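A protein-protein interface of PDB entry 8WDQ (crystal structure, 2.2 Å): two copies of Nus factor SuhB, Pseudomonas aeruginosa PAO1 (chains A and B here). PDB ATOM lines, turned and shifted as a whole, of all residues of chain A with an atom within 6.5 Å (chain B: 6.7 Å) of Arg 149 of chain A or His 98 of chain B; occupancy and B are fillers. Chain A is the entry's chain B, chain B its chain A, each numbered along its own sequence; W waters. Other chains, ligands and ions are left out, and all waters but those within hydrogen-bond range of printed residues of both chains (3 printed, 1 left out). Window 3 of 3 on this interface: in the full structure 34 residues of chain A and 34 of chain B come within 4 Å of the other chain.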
ATOM      1  N   VAL A 146     -15.149   0.785  24.144  1.00  0.00           N
ATOM      2  CA  VAL A 146     -14.721   0.912  22.757  1.00  0.00           C
ATOM      3  C   VAL A 146     -14.410   2.382  22.468  1.00  0.00           C
ATOM      4  O   VAL A 146     -14.877   3.296  23.161  1.00  0.00           O
ATOM      5  CB  VAL A 146     -15.774   0.372  21.776  1.00  0.00           C
ATOM      6  CG1 VAL A 146     -15.931  -1.120  21.944  1.00  0.00           C
ATOM      7  CG2 VAL A 146     -17.127   1.108  21.949  1.00  0.00           C
ATOM      8  N   SER A 147     -13.605   2.609  21.430  1.00  0.00           N
ATOM      9  CA  SER A 147     -13.231   3.975  21.093  1.00  0.00           C
ATOM     10  C   SER A 147     -14.457   4.761  20.630  1.00  0.00           C
ATOM     11  O   SER A 147     -15.529   4.203  20.364  1.00  0.00           O
ATOM     12  CB  SER A 147     -12.141   3.988  20.020  1.00  0.00           C
ATOM     13  OG  SER A 147     -12.678   3.729  18.734  1.00  0.00           O
ATOM     14  N   GLY A 148     -14.295   6.079  20.552  1.00  0.00           N
ATOM     15  CA  GLY A 148     -15.361   6.965  20.147  1.00  0.00           C
ATOM     16  C   GLY A 148     -15.303   7.447  18.718  1.00  0.00           C
ATOM     17  O   GLY A 148     -16.196   8.190  18.298  1.00  0.00           O
ATOM     18  N   ARG A 149     -14.287   7.042  17.955  1.00  0.00           N
ATOM     19  CA  ARG A 149     -14.118   7.498  16.579  1.00  0.00           C
ATOM     20  C   ARG A 149     -15.403   7.340  15.775  1.00  0.00           C
ATOM     21  O   ARG A 149     -16.049   6.290  15.810  1.00  0.00           O
ATOM     22  CB  ARG A 149     -12.981   6.721  15.911  1.00  0.00           C
ATOM     23  CG  ARG A 149     -12.577   7.265  14.551  1.00  0.00           C
ATOM     24  CD  ARG A 149     -11.348   6.538  14.038  1.00  0.00           C
ATOM     25  NE  ARG A 149     -10.196   6.805  14.889  1.00  0.00           N
ATOM     26  CZ  ARG A 149      -9.457   7.902  14.816  1.00  0.00           C
ATOM     27  NH1 ARG A 149      -9.693   8.834  13.908  1.00  0.00           N
ATOM     28  NH2 ARG A 149      -8.461   8.068  15.677  1.00  0.00           N
ATOM     29  N   LYS A 150     -15.761   8.395  15.038  1.00  0.00           N
ATOM     30  CA  LYS A 150     -17.053   8.497  14.377  1.00  0.00           C
ATOM     31  C   LYS A 150     -17.075   7.926  12.964  1.00  0.00           C
ATOM     32  O   LYS A 150     -18.160   7.785  12.394  1.00  0.00           O
ATOM     33  CB  LYS A 150     -17.497   9.968  14.331  1.00  0.00           C
ATOM     34  CG  LYS A 150     -17.739  10.572  15.699  1.00  0.00           C
ATOM     35  CD  LYS A 150     -19.114  10.200  16.234  1.00  0.00           C
ATOM     36  CE  LYS A 150     -19.262  10.631  17.687  1.00  0.00           C
ATOM     37  NZ  LYS A 150     -18.971   9.493  18.623  1.00  0.00           N
ATOM     38  N   SER A 151     -15.924   7.616  12.377  1.00  0.00           N
ATOM     39  CA  SER A 151     -15.867   7.084  11.019  1.00  0.00           C
ATOM     40  C   SER A 151     -14.513   6.408  10.833  1.00  0.00           C
ATOM     41  O   SER A 151     -13.679   6.389  11.742  1.00  0.00           O
ATOM     42  CB  SER A 151     -16.081   8.188   9.980  1.00  0.00           C
ATOM     43  OG  SER A 151     -14.896   8.965   9.858  1.00  0.00           O
ATOM     44  N   LEU A 152     -14.295   5.856   9.637  1.00  0.00           N
ATOM     45  CA  LEU A 152     -13.015   5.217   9.351  1.00  0.00           C
ATOM     46  C   LEU A 152     -11.895   6.224   9.111  1.00  0.00           C
ATOM     47  O   LEU A 152     -10.740   5.812   8.965  1.00  0.00           O
ATOM     48  CB  LEU A 152     -13.144   4.281   8.143  1.00  0.00           C
ATOM     49  CG  LEU A 152     -14.129   3.118   8.302  1.00  0.00           C
ATOM     50  CD1 LEU A 152     -14.150   2.227   7.063  1.00  0.00           C
ATOM     51  CD2 LEU A 152     -13.789   2.292   9.540  1.00  0.00           C
ATOM     52  N   GLU A 153     -12.203   7.521   9.063  1.00  0.00           N
ATOM     53  CA  GLU A 153     -11.174   8.542   8.906  1.00  0.00           C
ATOM     54  C   GLU A 153     -10.197   8.469  10.068  1.00  0.00           C
ATOM     55  O   GLU A 153     -10.583   8.685  11.223  1.00  0.00           O
ATOM     56  CB  GLU A 153     -11.814   9.930   8.850  1.00  0.00           C
ATOM     57  CG  GLU A 153     -12.505  10.277   7.537  1.00  0.00           C
ATOM     58  CD  GLU A 153     -11.609  10.173   6.308  1.00  0.00           C
ATOM     59  OE1 GLU A 153     -10.374  10.371   6.413  1.00  0.00           O
ATOM     60  OE2 GLU A 153     -12.161   9.885   5.226  1.00  0.00           O
ATOM     61  N   GLY A 154      -8.935   8.161   9.766  1.00  0.00           N
ATOM     62  CA  GLY A 154      -7.922   8.019  10.789  1.00  0.00           C
ATOM     63  C   GLY A 154      -8.049   6.786  11.656  1.00  0.00           C
ATOM     64  O   GLY A 154      -7.355   6.691  12.675  1.00  0.00           O
ATOM     65  N   ALA A 155      -8.909   5.837  11.286  1.00  0.00           N
ATOM     66  CA  ALA A 155      -9.111   4.642  12.096  1.00  0.00           C
ATOM     67  C   ALA A 155      -7.909   3.705  12.029  1.00  0.00           C
ATOM     68  O   ALA A 155      -7.202   3.630  11.022  1.00  0.00           O
ATOM     69  CB  ALA A 155     -10.361   3.890  11.641  1.00  0.00           C
ATOM     70  N   LEU A 156      -7.690   2.977  13.118  1.00  0.00           N
ATOM     71  CA  LEU A 156      -6.712   1.901  13.165  1.00  0.00           C
ATOM     72  C   LEU A 156      -7.485   0.591  13.205  1.00  0.00           C
ATOM     73  O   LEU A 156      -8.191   0.306  14.181  1.00  0.00           O
ATOM     74  CB  LEU A 156      -5.784   2.039  14.372  1.00  0.00           C
ATOM     75  CG  LEU A 156      -4.673   0.985  14.413  1.00  0.00           C
ATOM     76  CD1 LEU A 156      -3.698   1.174  13.249  1.00  0.00           C
ATOM     77  CD2 LEU A 156      -3.944   1.021  15.749  1.00  0.00           C
ATOM     78  N   LEU A 157      -7.365  -0.199  12.146  1.00  0.00           N
ATOM     79  CA  LEU A 157      -8.111  -1.443  12.048  1.00  0.00           C
ATOM     80  C   LEU A 157      -7.216  -2.633  12.355  1.00  0.00           C
ATOM     81  O   LEU A 157      -6.017  -2.625  12.069  1.00  0.00           O
ATOM     82  CB  LEU A 157      -8.719  -1.612  10.654  1.00  0.00           C
ATOM     83  CG  LEU A 157      -9.524  -0.436  10.112  1.00  0.00           C
ATOM     84  CD1 LEU A 157     -10.269  -0.870   8.869  1.00  0.00           C
ATOM     85  CD2 LEU A 157     -10.486   0.095  11.177  1.00  0.00           C
ATOM     86  N   ALA A 186      -5.915   5.304   9.198  1.00  0.00           N
ATOM     87  CA  ALA A 186      -4.538   5.633   9.537  1.00  0.00           C
ATOM     88  C   ALA A 186      -3.638   4.408   9.511  1.00  0.00           C
ATOM     89  O   ALA A 186      -2.418   4.547   9.379  1.00  0.00           O
ATOM     90  CB  ALA A 186      -4.469   6.293  10.913  1.00  0.00           C
ATOM     91  N   ALA A 203     -10.942  -2.649  24.113  1.00  0.00           N
ATOM     92  CA  ALA A 203     -10.267  -1.649  24.935  1.00  0.00           C
ATOM     93  C   ALA A 203     -10.131  -0.299  24.243  1.00  0.00           C
ATOM     94  O   ALA A 203      -9.618   0.644  24.860  1.00  0.00           O
ATOM     95  CB  ALA A 203      -8.880  -2.146  25.353  1.00  0.00           C
ATOM     96  N   GLY A 204     -10.571  -0.181  22.992  1.00  0.00           N
ATOM     97  CA  GLY A 204     -10.420   1.055  22.250  1.00  0.00           C
ATOM     98  C   GLY A 204      -9.115   1.191  21.504  1.00  0.00           C
ATOM     99  O   GLY A 204      -8.833   2.272  20.974  1.00  0.00           O
ATOM    100  N   ARG A 205      -8.312   0.126  21.442  1.00  0.00           N
ATOM    101  CA  ARG A 205      -7.009   0.184  20.786  1.00  0.00           C
ATOM    102  C   ARG A 205      -7.126   0.018  19.276  1.00  0.00           C
ATOM    103  O   ARG A 205      -6.335   0.600  18.526  1.00  0.00           O
ATOM    104  CB  ARG A 205      -6.090  -0.884  21.367  1.00  0.00           C
ATOM    105  CG  ARG A 205      -5.992  -0.831  22.884  1.00  0.00           C
ATOM    106  CD  ARG A 205      -5.015  -1.870  23.385  1.00  0.00           C
ATOM    107  NE  ARG A 205      -4.553  -1.598  24.741  1.00  0.00           N
ATOM    108  CZ  ARG A 205      -3.884  -2.475  25.477  1.00  0.00           C
ATOM    109  NH1 ARG A 205      -3.594  -3.685  25.013  1.00  0.00           N
ATOM    110  NH2 ARG A 205      -3.490  -2.130  26.701  1.00  0.00           N
ATOM    111  N   TYR A 206      -8.068  -0.804  18.820  1.00  0.00           N
ATOM    112  CA  TYR A 206      -8.493  -0.840  17.429  1.00  0.00           C
ATOM    113  C   TYR A 206      -9.900  -0.271  17.337  1.00  0.00           C
ATOM    114  O   TYR A 206     -10.716  -0.441  18.247  1.00  0.00           O
ATOM    115  CB  TYR A 206      -8.498  -2.259  16.855  1.00  0.00           C
ATOM    116  CG  TYR A 206      -7.142  -2.910  16.692  1.00  0.00           C
ATOM    117  CD1 TYR A 206      -5.977  -2.155  16.645  1.00  0.00           C
ATOM    118  CD2 TYR A 206      -7.037  -4.290  16.579  1.00  0.00           C
ATOM    119  CE1 TYR A 206      -4.740  -2.763  16.491  1.00  0.00           C
ATOM    120  CE2 TYR A 206      -5.814  -4.907  16.429  1.00  0.00           C
ATOM    121  CZ  TYR A 206      -4.668  -4.145  16.386  1.00  0.00           C
ATOM    122  OH  TYR A 206      -3.456  -4.786  16.233  1.00  0.00           O
ATOM    123  N   ASP A 207     -10.181   0.409  16.235  1.00  0.00           N
ATOM    124  CA  ASP A 207     -11.525   0.921  16.031  1.00  0.00           C
ATOM    125  C   ASP A 207     -12.447  -0.112  15.412  1.00  0.00           C
ATOM    126  O   ASP A 207     -13.671  -0.011  15.573  1.00  0.00           O
ATOM    127  CB  ASP A 207     -11.475   2.184  15.173  1.00  0.00           C
ATOM    128  CG  ASP A 207     -10.555   3.229  15.759  1.00  0.00           C
ATOM    129  OD1 ASP A 207     -10.767   3.598  16.930  1.00  0.00           O
ATOM    130  OD2 ASP A 207      -9.613   3.671  15.067  1.00  0.00           O
ATOM    131  N   ASN A 252     -16.158  -0.507  17.275  1.00  0.00           N
ATOM    132  CA  ASN A 252     -17.017   0.490  17.885  1.00  0.00           C
ATOM    133  C   ASN A 252     -18.233   0.687  16.979  1.00  0.00           C
ATOM    134  O   ASN A 252     -18.303   0.140  15.881  1.00  0.00           O
ATOM    135  CB  ASN A 252     -16.231   1.782  18.172  1.00  0.00           C
ATOM    136  CG  ASN A 252     -16.049   2.694  16.951  1.00  0.00           C
ATOM    137  OD1 ASN A 252     -16.589   2.462  15.874  1.00  0.00           O
ATOM    138  ND2 ASN A 252     -15.274   3.762  17.140  1.00  0.00           N
ATOM    139  N   THR A 253     -19.202   1.478  17.442  1.00  0.00           N
ATOM    140  CA  THR A 253     -20.482   1.554  16.737  1.00  0.00           C
ATOM    141  C   THR A 253     -20.299   1.968  15.279  1.00  0.00           C
ATOM    142  O   THR A 253     -20.625   1.210  14.348  1.00  0.00           O
ATOM    143  CB  THR A 253     -21.421   2.519  17.465  1.00  0.00           C
ATOM    144  OG1 THR A 253     -21.413   2.224  18.870  1.00  0.00           O
ATOM    145  CG2 THR A 253     -22.841   2.384  16.926  1.00  0.00           C
ATOM    146  N   LYS A 254     -19.738   3.160  15.059  1.00  0.00           N
ATOM    147  CA  LYS A 254     -19.710   3.711  13.711  1.00  0.00           C
ATOM    148  C   LYS A 254     -18.714   2.975  12.821  1.00  0.00           C
ATOM    149  O   LYS A 254     -18.986   2.759  11.633  1.00  0.00           O
ATOM    150  CB  LYS A 254     -19.400   5.206  13.764  1.00  0.00           C
ATOM    151  CG  LYS A 254     -20.403   5.997  14.606  1.00  0.00           C
ATOM    152  CD  LYS A 254     -21.101   7.065  13.783  1.00  0.00           C
ATOM    153  CE  LYS A 254     -22.478   6.584  13.359  1.00  0.00           C
ATOM    154  NZ  LYS A 254     -23.373   7.694  12.905  1.00  0.00           N
ATOM    155  N   CYS A 255     -17.562   2.575  13.369  1.00  0.00           N
ATOM    156  CA  CYS A 255     -16.570   1.887  12.549  1.00  0.00           C
ATOM    157  C   CYS A 255     -16.974   0.443  12.268  1.00  0.00           C
ATOM    158  O   CYS A 255     -16.676  -0.071  11.186  1.00  0.00           O
ATOM    159  CB  CYS A 255     -15.187   1.953  13.201  1.00  0.00           C
ATOM    160  SG  CYS A 255     -14.444   3.625  13.144  1.00  0.00           S
ATOM    161  N   ILE B  25       1.927   6.036  28.144  1.00  0.00           N
ATOM    162  CA  ILE B  25       0.928   5.067  27.693  1.00  0.00           C
ATOM    163  C   ILE B  25       0.237   4.420  28.889  1.00  0.00           C
ATOM    164  O   ILE B  25      -0.969   4.147  28.858  1.00  0.00           O
ATOM    165  CB  ILE B  25       1.574   4.016  26.766  1.00  0.00           C
ATOM    166  CG1 ILE B  25       0.522   3.052  26.226  1.00  0.00           C
ATOM    167  CG2 ILE B  25       2.655   3.231  27.485  1.00  0.00           C
ATOM    168  CD1 ILE B  25      -0.028   3.462  24.881  1.00  0.00           C
ATOM    169  N   TYR B  41       1.892  11.459  12.259  1.00  0.00           N
ATOM    170  CA  TYR B  41       1.564  12.128  13.510  1.00  0.00           C
ATOM    171  C   TYR B  41       2.817  12.460  14.311  1.00  0.00           C
ATOM    172  O   TYR B  41       3.813  11.729  14.282  1.00  0.00           O
ATOM    173  CB  TYR B  41       0.629  11.271  14.367  1.00  0.00           C
ATOM    174  CG  TYR B  41      -0.663  10.872  13.694  1.00  0.00           C
ATOM    175  CD1 TYR B  41      -1.050   9.537  13.621  1.00  0.00           C
ATOM    176  CD2 TYR B  41      -1.508  11.832  13.145  1.00  0.00           C
ATOM    177  CE1 TYR B  41      -2.241   9.170  13.010  1.00  0.00           C
ATOM    178  CE2 TYR B  41      -2.696  11.477  12.533  1.00  0.00           C
ATOM    179  CZ  TYR B  41      -3.059  10.147  12.468  1.00  0.00           C
ATOM    180  OH  TYR B  41      -4.243   9.800  11.857  1.00  0.00           O
ATOM    181  N   THR B  93       4.120   5.348  16.152  1.00  0.00           N
ATOM    182  CA  THR B  93       3.350   6.459  16.712  1.00  0.00           C
ATOM    183  C   THR B  93       1.841   6.228  16.606  1.00  0.00           C
ATOM    184  O   THR B  93       1.087   6.602  17.510  1.00  0.00           O
ATOM    185  CB  THR B  93       3.743   7.771  16.015  1.00  0.00           C
ATOM    186  OG1 THR B  93       5.098   8.114  16.351  1.00  0.00           O
ATOM    187  CG2 THR B  93       2.838   8.913  16.449  1.00  0.00           C
ATOM    188  N   THR B  94       1.374   5.630  15.510  1.00  0.00           N
ATOM    189  CA  THR B  94      -0.060   5.384  15.378  1.00  0.00           C
ATOM    190  C   THR B  94      -0.526   4.332  16.380  1.00  0.00           C
ATOM    191  O   THR B  94      -1.558   4.504  17.050  1.00  0.00           O
ATOM    192  CB  THR B  94      -0.384   4.979  13.941  1.00  0.00           C
ATOM    193  OG1 THR B  94       0.134   5.979  13.051  1.00  0.00           O
ATOM    194  CG2 THR B  94      -1.894   4.851  13.726  1.00  0.00           C
ATOM    195  N   ASN B  95       0.237   3.240  16.505  1.00  0.00           N
ATOM    196  CA  ASN B  95       0.032   2.295  17.599  1.00  0.00           C
ATOM    197  C   ASN B  95      -0.058   3.029  18.931  1.00  0.00           C
ATOM    198  O   ASN B  95      -1.015   2.846  19.692  1.00  0.00           O
ATOM    199  CB  ASN B  95       1.172   1.269  17.635  1.00  0.00           C
ATOM    200  CG  ASN B  95       0.999   0.149  16.612  1.00  0.00           C
ATOM    201  OD1 ASN B  95       0.040   0.137  15.840  1.00  0.00           O
ATOM    202  ND2 ASN B  95       1.928  -0.803  16.612  1.00  0.00           N
ATOM    203  N   PHE B  96       0.927   3.886  19.215  1.00  0.00           N
ATOM    204  CA  PHE B  96       0.971   4.560  20.509  1.00  0.00           C
ATOM    205  C   PHE B  96      -0.286   5.390  20.741  1.00  0.00           C
ATOM    206  O   PHE B  96      -0.937   5.267  21.785  1.00  0.00           O
ATOM    207  CB  PHE B  96       2.213   5.446  20.618  1.00  0.00           C
ATOM    208  CG  PHE B  96       2.271   6.236  21.898  1.00  0.00           C
ATOM    209  CD1 PHE B  96       2.788   5.669  23.051  1.00  0.00           C
ATOM    210  CD2 PHE B  96       1.789   7.533  21.957  1.00  0.00           C
ATOM    211  CE1 PHE B  96       2.836   6.383  24.234  1.00  0.00           C
ATOM    212  CE2 PHE B  96       1.834   8.250  23.138  1.00  0.00           C
ATOM    213  CZ  PHE B  96       2.357   7.673  24.278  1.00  0.00           C
ATOM    214  N   ILE B  97      -0.645   6.242  19.772  1.00  0.00           N
ATOM    215  CA  ILE B  97      -1.776   7.147  19.966  1.00  0.00           C
ATOM    216  C   ILE B  97      -3.065   6.350  20.121  1.00  0.00           C
ATOM    217  O   ILE B  97      -4.010   6.805  20.780  1.00  0.00           O
ATOM    218  CB  ILE B  97      -1.863   8.176  18.813  1.00  0.00           C
ATOM    219  CG1 ILE B  97      -2.997   9.179  19.043  1.00  0.00           C
ATOM    220  CG2 ILE B  97      -2.102   7.505  17.483  1.00  0.00           C
ATOM    221  CD1 ILE B  97      -3.058   9.729  20.452  1.00  0.00           C
ATOM    222  N   HIS B  98      -3.122   5.145  19.555  1.00  0.00           N
ATOM    223  CA  HIS B  98      -4.281   4.293  19.796  1.00  0.00           C
ATOM    224  C   HIS B  98      -4.153   3.454  21.063  1.00  0.00           C
ATOM    225  O   HIS B  98      -5.116   2.778  21.441  1.00  0.00           O
ATOM    226  CB  HIS B  98      -4.534   3.397  18.581  1.00  0.00           C
ATOM    227  CG  HIS B  98      -5.153   4.128  17.434  1.00  0.00           C
ATOM    228  ND1 HIS B  98      -6.507   4.107  17.182  1.00  0.00           N
ATOM    229  CD2 HIS B  98      -4.610   4.944  16.501  1.00  0.00           C
ATOM    230  CE1 HIS B  98      -6.768   4.862  16.130  1.00  0.00           C
ATOM    231  NE2 HIS B  98      -5.633   5.380  15.697  1.00  0.00           N
ATOM    232  N   GLY B  99      -3.008   3.496  21.743  1.00  0.00           N
ATOM    233  CA  GLY B  99      -2.814   2.669  22.919  1.00  0.00           C
ATOM    234  C   GLY B  99      -2.423   1.237  22.634  1.00  0.00           C
ATOM    235  O   GLY B  99      -2.471   0.403  23.546  1.00  0.00           O
ATOM    236  N   VAL B 100      -2.056   0.919  21.396  1.00  0.00           N
ATOM    237  CA  VAL B 100      -1.578  -0.413  21.037  1.00  0.00           C
ATOM    238  C   VAL B 100      -0.169  -0.563  21.594  1.00  0.00           C
ATOM    239  O   VAL B 100       0.729   0.198  21.212  1.00  0.00           O
ATOM    240  CB  VAL B 100      -1.609  -0.625  19.517  1.00  0.00           C
ATOM    241  CG1 VAL B 100      -0.983  -1.966  19.156  1.00  0.00           C
ATOM    242  CG2 VAL B 100      -3.041  -0.529  18.990  1.00  0.00           C
ATOM    243  N   PRO B 101       0.072  -1.508  22.503  1.00  0.00           N
ATOM    244  CA  PRO B 101       1.378  -1.595  23.184  1.00  0.00           C
ATOM    245  C   PRO B 101       2.436  -2.305  22.343  1.00  0.00           C
ATOM    246  O   PRO B 101       2.949  -3.374  22.703  1.00  0.00           O
ATOM    247  CB  PRO B 101       1.025  -2.364  24.463  1.00  0.00           C
ATOM    248  CG  PRO B 101      -0.080  -3.296  24.021  1.00  0.00           C
ATOM    249  CD  PRO B 101      -0.872  -2.541  22.970  1.00  0.00           C
HETATM  250  O   HOH W   1      -0.699   6.538  10.621  1.00  0.00           O
HETATM  251  O   HOH W   2      -5.249   7.582  14.140  1.00  0.00           O
HETATM  252  O   HOH W   3      -1.825   0.540  26.176  1.00  0.00           O
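Arg 149 of chain A touches just one residue of chain B: His 98 (3.7 Å). Printed residues of chain B within 4 Å of Gly 154 of chain A: His 98. Printed residues of chain B within 4 Å of Gly 204 of chain A: His 98 (3.8 Å). Of the printed residues of chain B, Arg 205 of chain A touches His 98, Gly 99, Val 100 and Pro 101. Of the printed residues of chain B, Tyr 206 of chain A touches Val 100 (3.8 Å). Printed residues of chain B within 4 Å of Asp 207 of chain A: His 98. Of chain A, only Arg 149, Gly 154, Leu 156, Gly 204, Arg 205 and Asp 207 come within 4 Å of His 98 of chain B. The nearest residue of chain A that does not touch His 98 of chain B is Ala 155 of chain A (4.4 Å). The nearest printed residue of chain B that does not touch Gly 154 of chain A is Tyr 41 of chain B (4.2 Å).
O of Gly 99 of chain B is in hydrogen-bond range of NE of Arg 205 of chain A (3.1 Å).
No position is printed for both chains.
The backbone NH of Val 100 of chain B lies within hydrogen-bond range of the backbone carbonyl oxygen of Asn 95 of chain B. The side-chain carboxylate (OD1) of Asp 207 of chain A lies within hydrogen-bond range of the side-chain hydroxyl (OG) of Ser 147 of chain A, 2.6 Å away. The guanidinium group of Arg 149 of chain A lies close to the backbone carbonyl oxygen of Gly 154 of chain A (3.4 Å). The backbone carbonyl oxygen (O) of Arg 149 of chain A lies within hydrogen-bond range of the side-chain amide nitrogen (ND2) of Asn 252 of chain A (3.0 Å). The backbone NH of Leu 156 of chain A sits at hydrogen-bond distance from the side-chain carboxylate of Asp 207 of chain A (2.8 Å). O of Asp 207 of chain A sits at hydrogen-bond distance from N of Asn 252 of chain A, 3.1 Å away.
Water W1 lies within hydrogen-bond range of the side-chain hydroxyl (OG1) of Thr 94 of chain B and the backbone carbonyl oxygen (O) of Ala 186 of chain A. Water W3 bridges the backbone carbonyl oxygen of Gly 99 of chain B (2.7 Å) and the guanidinium group of Arg 205 of chain A (3.2 Å). Water W2 lies within hydrogen-bond range of the backbone carbonyl oxygen (O) of Gly 154 of chain A (2.7 Å), a ring nitrogen (NE2) of His 98 of chain B (2.7 Å) and the side-chain hydroxyl (OH) of Tyr 41 of chain B (3.3 Å).
Among the printed residues, pairs that only touch across the chains: Arg 149 of chain A with His 98 of chain B (3.7 Å), Gly 154 of chain A with His 98 of chain B (3.7 Å), Leu 156 of chain A with His 98 of chain B (3.5 Å), Leu 156 of chain A with Val 100 of chain B (3.7 Å), Ala 186 of chain A with Tyr 41 of chain B (3.6 Å), Gly 204 of chain A with His 98 of chain B (3.8 Å), Arg 205 of chain A with His 98 of chain B (3.3 Å), Arg 205 of chain A with Val 100 of chain B (3.5 Å), Arg 205 of chain A with Pro 101 of chain B (3.6 Å), Tyr 206 of chain A with Val 100 of chain B (3.8 Å) and Asp 207 of chain A with His 98 of chain B (3.3 Å).
Printed residues of chain B that touch a printed residue of chain A: Tyr 41, His 98, Gly 99, Val 100 and Pro 101. Hydrophobic or aromatic side chains of chain B that line the printed part of chain A: Tyr 41, His 98, Val 100 and Pro 101. Along chain B the printed residues that touch a printed residue of chain A span positions 41 to 101. Of the 22 printed residues of chain A, 8 touch a printed residue of chain B.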
